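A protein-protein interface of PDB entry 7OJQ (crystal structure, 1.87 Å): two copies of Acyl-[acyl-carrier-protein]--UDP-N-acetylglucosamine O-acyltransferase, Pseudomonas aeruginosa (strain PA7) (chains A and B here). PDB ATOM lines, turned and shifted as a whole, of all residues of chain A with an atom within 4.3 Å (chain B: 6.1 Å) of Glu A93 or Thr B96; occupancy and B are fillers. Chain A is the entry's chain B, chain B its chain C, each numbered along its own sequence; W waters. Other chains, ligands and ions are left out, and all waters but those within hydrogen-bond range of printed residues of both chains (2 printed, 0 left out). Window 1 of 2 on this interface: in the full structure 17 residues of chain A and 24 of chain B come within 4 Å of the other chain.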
ATOM      1  N   TYR A  62      -6.870  -1.788  -0.294  1.00  0.00           N
ATOM      2  CA  TYR A  62      -7.111  -0.488   0.343  1.00  0.00           C
ATOM      3  C   TYR A  62      -6.139   0.604  -0.109  1.00  0.00           C
ATOM      4  O   TYR A  62      -5.099   0.317  -0.708  1.00  0.00           O
ATOM      5  CB  TYR A  62      -7.109  -0.630   1.873  1.00  0.00           C
ATOM      6  CG  TYR A  62      -8.384  -1.258   2.397  1.00  0.00           C
ATOM      7  CD1 TYR A  62      -8.667  -2.606   2.171  1.00  0.00           C
ATOM      8  CD2 TYR A  62      -9.321  -0.500   3.100  1.00  0.00           C
ATOM      9  CE1 TYR A  62      -9.832  -3.195   2.666  1.00  0.00           C
ATOM     10  CE2 TYR A  62     -10.508  -1.071   3.568  1.00  0.00           C
ATOM     11  CZ  TYR A  62     -10.748  -2.422   3.363  1.00  0.00           C
ATOM     12  OH  TYR A  62     -11.894  -2.995   3.849  1.00  0.00           O
ATOM     13  N   GLN A  63      -6.496   1.860   0.212  1.00  0.00           N
ATOM     14  CA  GLN A  63      -5.765   3.092  -0.113  1.00  0.00           C
ATOM     15  C   GLN A  63      -4.290   3.075   0.257  1.00  0.00           C
ATOM     16  O   GLN A  63      -3.908   2.521   1.297  1.00  0.00           O
ATOM     17  CB  GLN A  63      -6.434   4.306   0.568  1.00  0.00           C
ATOM     18  CG  GLN A  63      -6.566   4.188   2.093  1.00  0.00           C
ATOM     19  CD  GLN A  63      -7.843   3.553   2.572  1.00  0.00           C
ATOM     20  OE1 GLN A  63      -8.589   2.948   1.811  1.00  0.00           O
ATOM     21  NE2 GLN A  63      -8.117   3.677   3.856  1.00  0.00           N
ATOM     22  N   SER A  65      -1.702   1.696  -1.175  1.00  0.00           N
ATOM     23  CA  SER A  65      -0.998   0.446  -1.459  1.00  0.00           C
ATOM     24  C   SER A  65      -0.298   0.584  -2.773  1.00  0.00           C
ATOM     25  O   SER A  65      -0.793   1.282  -3.656  1.00  0.00           O
ATOM     26  CB  SER A  65      -1.977  -0.727  -1.521  1.00  0.00           C
ATOM     27  OG  SER A  65      -2.338  -1.125  -0.212  1.00  0.00           O
ATOM     28  N   ARG A  92      -4.613  -4.459   2.996  1.00  0.00           N
ATOM     29  CA  ARG A  92      -4.944  -3.237   3.706  1.00  0.00           C
ATOM     30  C   ARG A  92      -4.082  -2.040   3.258  1.00  0.00           C
ATOM     31  O   ARG A  92      -3.348  -2.125   2.268  1.00  0.00           O
ATOM     32  CB  ARG A  92      -4.922  -3.454   5.234  1.00  0.00           C
ATOM     33  CG  ARG A  92      -5.953  -4.503   5.739  1.00  0.00           C
ATOM     34  CD  ARG A  92      -7.405  -4.046   5.687  1.00  0.00           C
ATOM     35  NE  ARG A  92      -7.598  -2.776   6.388  1.00  0.00           N
ATOM     36  CZ  ARG A  92      -8.757  -2.356   6.893  1.00  0.00           C
ATOM     37  NH1 ARG A  92      -9.849  -3.103   6.780  1.00  0.00           N
ATOM     38  NH2 ARG A  92      -8.831  -1.191   7.520  1.00  0.00           N
ATOM     39  N   GLU A  93      -4.267  -0.894   3.920  1.00  0.00           N
ATOM     40  CA  GLU A  93      -3.607   0.362   3.601  1.00  0.00           C
ATOM     41  C   GLU A  93      -2.103   0.311   3.638  1.00  0.00           C
ATOM     42  O   GLU A  93      -1.536  -0.268   4.556  1.00  0.00           O
ATOM     43  CB  GLU A  93      -4.110   1.532   4.494  1.00  0.00           C
ATOM     44  CG  GLU A  93      -4.173   1.285   6.003  1.00  0.00           C
ATOM     45  CD  GLU A  93      -5.256   0.393   6.613  1.00  0.00           C
ATOM     46  OE1 GLU A  93      -6.037  -0.232   5.860  1.00  0.00           O
ATOM     47  OE2 GLU A  93      -5.311   0.306   7.862  1.00  0.00           O
ATOM     48  N   GLY A  94      -1.471   0.961   2.665  1.00  0.00           N
ATOM     49  CA  GLY A  94      -0.015   1.104   2.623  1.00  0.00           C
ATOM     50  C   GLY A  94       0.806  -0.148   2.369  1.00  0.00           C
ATOM     51  O   GLY A  94       2.024  -0.121   2.546  1.00  0.00           O
ATOM     52  N   VAL A  95       0.177  -1.256   1.970  1.00  0.00           N
ATOM     53  CA  VAL A  95       0.933  -2.499   1.727  1.00  0.00           C
ATOM     54  C   VAL A  95       1.763  -2.353   0.478  1.00  0.00           C
ATOM     55  O   VAL A  95       1.278  -1.777  -0.485  1.00  0.00           O
ATOM     56  CB  VAL A  95      -0.006  -3.740   1.669  1.00  0.00           C
ATOM     57  CG1 VAL A  95       0.682  -4.986   1.061  1.00  0.00           C
ATOM     58  CG2 VAL A  95      -0.622  -4.050   3.036  1.00  0.00           C
ATOM     59  N   ALA A 118      -2.165  -3.597   7.307  1.00  0.00           N
ATOM     60  CA  ALA A 118      -1.569  -2.283   7.080  1.00  0.00           C
ATOM     61  C   ALA A 118      -0.047  -2.244   7.115  1.00  0.00           C
ATOM     62  O   ALA A 118       0.570  -2.663   8.095  1.00  0.00           O
ATOM     63  CB  ALA A 118      -2.152  -1.247   8.037  1.00  0.00           C
ATOM     64  N   TYR A 119       0.540  -1.729   6.020  1.00  0.00           N
ATOM     65  CA  TYR A 119       1.983  -1.485   5.846  1.00  0.00           C
ATOM     66  C   TYR A 119       2.856  -2.732   5.830  1.00  0.00           C
ATOM     67  O   TYR A 119       4.081  -2.623   5.966  1.00  0.00           O
ATOM     68  CB  TYR A 119       2.521  -0.472   6.878  1.00  0.00           C
ATOM     69  CG  TYR A 119       1.762   0.827   6.796  1.00  0.00           C
ATOM     70  CD1 TYR A 119       1.929   1.689   5.709  1.00  0.00           C
ATOM     71  CD2 TYR A 119       0.813   1.159   7.752  1.00  0.00           C
ATOM     72  CE1 TYR A 119       1.187   2.864   5.597  1.00  0.00           C
ATOM     73  CE2 TYR A 119       0.104   2.362   7.679  1.00  0.00           C
ATOM     74  CZ  TYR A 119       0.289   3.206   6.592  1.00  0.00           C
ATOM     75  OH  TYR A 119      -0.430   4.365   6.494  1.00  0.00           O
ATOM     76  N   PHE B  64      -2.153  10.941   3.888  1.00  0.00           N
ATOM     77  CA  PHE B  64      -2.017   9.477   3.841  1.00  0.00           C
ATOM     78  C   PHE B  64      -2.480   8.768   5.126  1.00  0.00           C
ATOM     79  O   PHE B  64      -2.255   7.583   5.274  1.00  0.00           O
ATOM     80  CB  PHE B  64      -0.567   9.047   3.424  1.00  0.00           C
ATOM     81  CG  PHE B  64      -0.003   9.905   2.314  1.00  0.00           C
ATOM     82  CD1 PHE B  64      -0.708  10.095   1.130  1.00  0.00           C
ATOM     83  CD2 PHE B  64       1.234  10.528   2.452  1.00  0.00           C
ATOM     84  CE1 PHE B  64      -0.184  10.897   0.105  1.00  0.00           C
ATOM     85  CE2 PHE B  64       1.749  11.332   1.432  1.00  0.00           C
ATOM     86  CZ  PHE B  64       1.041  11.498   0.261  1.00  0.00           C
ATOM     87  N   SER B  65      -3.202   9.469   5.996  1.00  0.00           N
ATOM     88  CA  SER B  65      -3.811   8.907   7.205  1.00  0.00           C
ATOM     89  C   SER B  65      -5.170   8.298   6.839  1.00  0.00           C
ATOM     90  O   SER B  65      -5.835   8.762   5.911  1.00  0.00           O
ATOM     91  CB  SER B  65      -4.018  10.010   8.245  1.00  0.00           C
ATOM     92  OG  SER B  65      -2.786  10.299   8.886  1.00  0.00           O
ATOM     93  N   SER B  66      -5.564   7.252   7.555  1.00  0.00           N
ATOM     94  CA  SER B  66      -6.852   6.563   7.411  1.00  0.00           C
ATOM     95  C   SER B  66      -7.431   6.548   8.812  1.00  0.00           C
ATOM     96  O   SER B  66      -6.984   5.803   9.694  1.00  0.00           O
ATOM     97  CB  SER B  66      -6.665   5.150   6.863  1.00  0.00           C
ATOM     98  OG  SER B  66      -6.052   5.145   5.584  1.00  0.00           O
ATOM     99  N   VAL B  67      -8.335   7.465   9.040  1.00  0.00           N
ATOM    100  CA  VAL B  67      -8.900   7.682  10.350  1.00  0.00           C
ATOM    101  C   VAL B  67     -10.382   7.261  10.315  1.00  0.00           C
ATOM    102  O   VAL B  67     -11.159   7.787   9.522  1.00  0.00           O
ATOM    103  CB  VAL B  67      -8.666   9.159  10.775  1.00  0.00           C
ATOM    104  CG1 VAL B  67      -9.390   9.486  12.074  1.00  0.00           C
ATOM    105  CG2 VAL B  67      -7.159   9.478  10.888  1.00  0.00           C
ATOM    106  N   GLU B  69     -11.372   3.694  10.154  1.00  0.00           N
ATOM    107  CA  GLU B  69     -11.536   2.462   9.384  1.00  0.00           C
ATOM    108  C   GLU B  69     -12.180   1.348  10.225  1.00  0.00           C
ATOM    109  O   GLU B  69     -12.198   1.427  11.466  1.00  0.00           O
ATOM    110  CB  GLU B  69     -10.186   1.976   8.811  1.00  0.00           C
ATOM    111  CG  GLU B  69      -9.474   2.953   7.884  1.00  0.00           C
ATOM    112  CD  GLU B  69     -10.197   3.368   6.615  1.00  0.00           C
ATOM    113  OE1 GLU B  69     -10.396   2.509   5.724  1.00  0.00           O
ATOM    114  OE2 GLU B  69     -10.538   4.568   6.503  1.00  0.00           O
ATOM    115  N   GLY B  94       0.153   9.005   7.492  1.00  0.00           N
ATOM    116  CA  GLY B  94      -0.019   7.562   7.497  1.00  0.00           C
ATOM    117  C   GLY B  94      -0.544   6.912   8.758  1.00  0.00           C
ATOM    118  O   GLY B  94      -0.480   5.703   8.881  1.00  0.00           O
ATOM    119  N   VAL B  95      -1.039   7.692   9.705  1.00  0.00           N
ATOM    120  CA  VAL B  95      -1.610   7.125  10.926  1.00  0.00           C
ATOM    121  C   VAL B  95      -2.897   6.352  10.602  1.00  0.00           C
ATOM    122  O   VAL B  95      -3.690   6.803   9.776  1.00  0.00           O
ATOM    123  CB  VAL B  95      -1.852   8.258  11.962  1.00  0.00           C
ATOM    124  CG1 VAL B  95      -2.747   7.778  13.112  1.00  0.00           C
ATOM    125  CG2 VAL B  95      -0.501   8.757  12.497  1.00  0.00           C
ATOM    126  N   THR B  96      -3.074   5.161  11.211  1.00  0.00           N
ATOM    127  CA  THR B  96      -4.288   4.361  11.058  1.00  0.00           C
ATOM    128  C   THR B  96      -4.980   4.277  12.416  1.00  0.00           C
ATOM    129  O   THR B  96      -4.326   4.015  13.432  1.00  0.00           O
ATOM    130  CB  THR B  96      -3.978   2.991  10.421  1.00  0.00           C
ATOM    131  OG1 THR B  96      -3.021   2.297  11.227  1.00  0.00           O
ATOM    132  CG2 THR B  96      -3.476   3.120   8.973  1.00  0.00           C
ATOM    133  N   ILE B  97      -6.277   4.627  12.442  1.00  0.00           N
ATOM    134  CA  ILE B  97      -7.111   4.647  13.641  1.00  0.00           C
ATOM    135  C   ILE B  97      -8.396   3.920  13.298  1.00  0.00           C
ATOM    136  O   ILE B  97      -9.069   4.282  12.335  1.00  0.00           O
ATOM    137  CB  ILE B  97      -7.363   6.087  14.195  1.00  0.00           C
ATOM    138  CG1 ILE B  97      -6.033   6.870  14.358  1.00  0.00           C
ATOM    139  CG2 ILE B  97      -8.166   6.051  15.512  1.00  0.00           C
ATOM    140  CD1 ILE B  97      -6.193   8.378  14.674  1.00  0.00           C
ATOM    141  N   HIS B  98      -8.689   2.850  14.051  1.00  0.00           N
ATOM    142  CA  HIS B  98      -9.880   2.028  13.846  1.00  0.00           C
ATOM    143  C   HIS B  98     -10.950   2.409  14.824  1.00  0.00           C
ATOM    144  O   HIS B  98     -10.654   2.852  15.933  1.00  0.00           O
ATOM    145  CB  HIS B  98      -9.535   0.540  13.944  1.00  0.00           C
ATOM    146  CG  HIS B  98      -8.673   0.067  12.818  1.00  0.00           C
ATOM    147  ND1 HIS B  98      -9.011  -1.028  12.082  1.00  0.00           N
ATOM    148  CD2 HIS B  98      -7.544   0.592  12.305  1.00  0.00           C
ATOM    149  CE1 HIS B  98      -8.038  -1.183  11.196  1.00  0.00           C
ATOM    150  NE2 HIS B  98      -7.179  -0.197  11.256  1.00  0.00           N
ATOM    151  N   TYR B 119       2.757   7.017  10.919  1.00  0.00           N
ATOM    152  CA  TYR B 119       2.530   5.564  10.807  1.00  0.00           C
ATOM    153  C   TYR B 119       2.178   4.888  12.113  1.00  0.00           C
ATOM    154  O   TYR B 119       2.168   3.687  12.175  1.00  0.00           O
ATOM    155  CB  TYR B 119       3.721   4.857  10.099  1.00  0.00           C
ATOM    156  CG  TYR B 119       3.896   5.447   8.726  1.00  0.00           C
ATOM    157  CD1 TYR B 119       2.902   5.314   7.760  1.00  0.00           C
ATOM    158  CD2 TYR B 119       5.017   6.211   8.412  1.00  0.00           C
ATOM    159  CE1 TYR B 119       3.030   5.905   6.507  1.00  0.00           C
ATOM    160  CE2 TYR B 119       5.132   6.848   7.176  1.00  0.00           C
ATOM    161  CZ  TYR B 119       4.134   6.700   6.230  1.00  0.00           C
ATOM    162  OH  TYR B 119       4.271   7.290   5.006  1.00  0.00           O
ATOM    163  N   ALA B 120       1.810   5.647  13.132  1.00  0.00           N
ATOM    164  CA  ALA B 120       1.348   5.004  14.349  1.00  0.00           C
ATOM    165  C   ALA B 120      -0.014   4.307  14.065  1.00  0.00           C
ATOM    166  O   ALA B 120      -0.739   4.672  13.122  1.00  0.00           O
ATOM    167  CB  ALA B 120       1.199   6.029  15.457  1.00  0.00           C
ATOM    168  N   HIS B 121      -0.309   3.262  14.845  1.00  0.00           N
ATOM    169  CA  HIS B 121      -1.526   2.489  14.707  1.00  0.00           C
ATOM    170  C   HIS B 121      -2.281   2.450  16.027  1.00  0.00           C
ATOM    171  O   HIS B 121      -1.713   2.102  17.072  1.00  0.00           O
ATOM    172  CB  HIS B 121      -1.207   1.053  14.225  1.00  0.00           C
ATOM    173  CG  HIS B 121      -2.406   0.168  14.215  1.00  0.00           C
ATOM    174  ND1 HIS B 121      -3.384   0.290  13.244  1.00  0.00           N
ATOM    175  CD2 HIS B 121      -2.785  -0.785  15.102  1.00  0.00           C
ATOM    176  CE1 HIS B 121      -4.299  -0.624  13.542  1.00  0.00           C
ATOM    177  NE2 HIS B 121      -3.986  -1.281  14.657  1.00  0.00           N
ATOM    178  N   ILE B 122      -3.550   2.830  15.965  1.00  0.00           N
ATOM    179  CA  ILE B 122      -4.479   2.783  17.089  1.00  0.00           C
ATOM    180  C   ILE B 122      -5.586   1.771  16.743  1.00  0.00           C
ATOM    181  O   ILE B 122      -6.503   2.030  15.924  1.00  0.00           O
ATOM    182  CB  ILE B 122      -4.972   4.196  17.512  1.00  0.00           C
ATOM    183  CG1 ILE B 122      -3.756   5.121  17.832  1.00  0.00           C
ATOM    184  CG2 ILE B 122      -5.947   4.114  18.707  1.00  0.00           C
ATOM    185  CD1 ILE B 122      -4.054   6.555  17.619  1.00  0.00           C
ATOM    186  N   GLY B 123      -5.448   0.589  17.350  1.00  0.00           N
ATOM    187  CA  GLY B 123      -6.362  -0.522  17.154  1.00  0.00           C
ATOM    188  C   GLY B 123      -7.689  -0.285  17.826  1.00  0.00           C
ATOM    189  O   GLY B 123      -7.793   0.502  18.776  1.00  0.00           O
HETATM  190  O   HOH W   1      -3.254   5.137   6.198  1.00  0.00           O
HETATM  191  O   HOH W   2      -0.444   5.518   4.111  1.00  0.00           O
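Tyr A119 touches Gly B94, but with the chains exchanged Gly A94 does not touch Tyr B119 (6.9 Å). Tyr A119 touches its own counterpart, Tyr B119.
Water W2 bridges OH of Tyr A119 (2.6 Å) and O of Phe B64 (3.0 Å). Water W1 lies within hydrogen-bond range of the backbone carbonyl oxygen of Phe B64 (2.8 Å), the side-chain hydroxyl of Ser B66 (2.9 Å) and the side-chain hydroxyl of Tyr A119 (2.9 Å).
Of the 9 printed residues of chain A, 4 touch a printed residue of chain B. Printed residues of chain A that touch a printed residue of chain B: Gln A63, Arg A92, Glu A93 and Tyr A119. Hydrophobic or aromatic side chains of chain A that line the printed part of chain B: Tyr A119. Printed residues of chain B that touch a printed residue of chain A: Phe B64, Ser B66, Glu B69, Gly B94, Thr B96, His B98 and Tyr B119. Hydrophobic or aromatic side chains of chain B that line the printed part of chain A: His B98 and Tyr B119. Among the printed residues, 10 pairs touch across the chains.
Among the printed residues, merely in contact across the chains: Arg A92 with Glu B69, Arg A92 with His B98, Glu A93 with Thr B96, Glu A93 with His B98, Tyr A119 with Phe B64, Tyr A119 with Thr B96 and Tyr A119 with Tyr B119.
The backbone NH (N) of Gly A94 lies within hydrogen-bond range of the backbone carbonyl oxygen (O) of Gln A63, 3.2 Å away. OE1 of Glu A93 lies within salt-bridge range of NE of Arg A92. The backbone carbonyl oxygen (O) of Glu A93 sits at hydrogen-bond distance from the backbone NH (N) of Tyr A119 (2.9 Å). The backbone carbonyl oxygen of Ile B97 is in hydrogen-bond range of the backbone NH of Glu B69 (3.2 Å). The backbone carbonyl oxygen of Thr B96 sits at hydrogen-bond distance from the backbone NH of Ile B122 (2.9 Å). O of Ile B122 lies within hydrogen-bond range of N of His B98 (3.0 Å).
Tyr A62 touches none of the printed residues of chain B. Of the printed residues of chain B, Tyr A119 touches Phe B64 (3.9 Å), Gly B94 (2.7 Å), Thr B96 (3.9 Å) and Tyr B119 (3.6 Å). Of the printed residues of chain A, Ser B66 touches Gln A63 (3.1 Å). Thr B96 touches just these residues of chain A: Glu A93 and Tyr A119. Ala B120 touches none of the printed residues of chain A. The nearest printed residue of chain B that does not touch Glu A93 is Ser B66 (4.2 Å). The nearest printed residue of chain A that does not touch Thr B96 is Ala A118 (4.7 Å). The nearest printed residue of chain A that does not touch Ser B66 is Glu A93 (4.2 Å).
The side-chain hydroxyl (OG) of Ser B66 sits at hydrogen-bond distance from the side-chain amide nitrogen (NE2) of Gln A63 (3.1 Å). NE2 of Gln A63 sits at hydrogen-bond distance from OE1 of Glu B69 (3.2 Å). The side-chain hydroxyl of Tyr A119 sits at hydrogen-bond distance from the backbone carbonyl oxygen of Gly B94 (2.7 Å).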
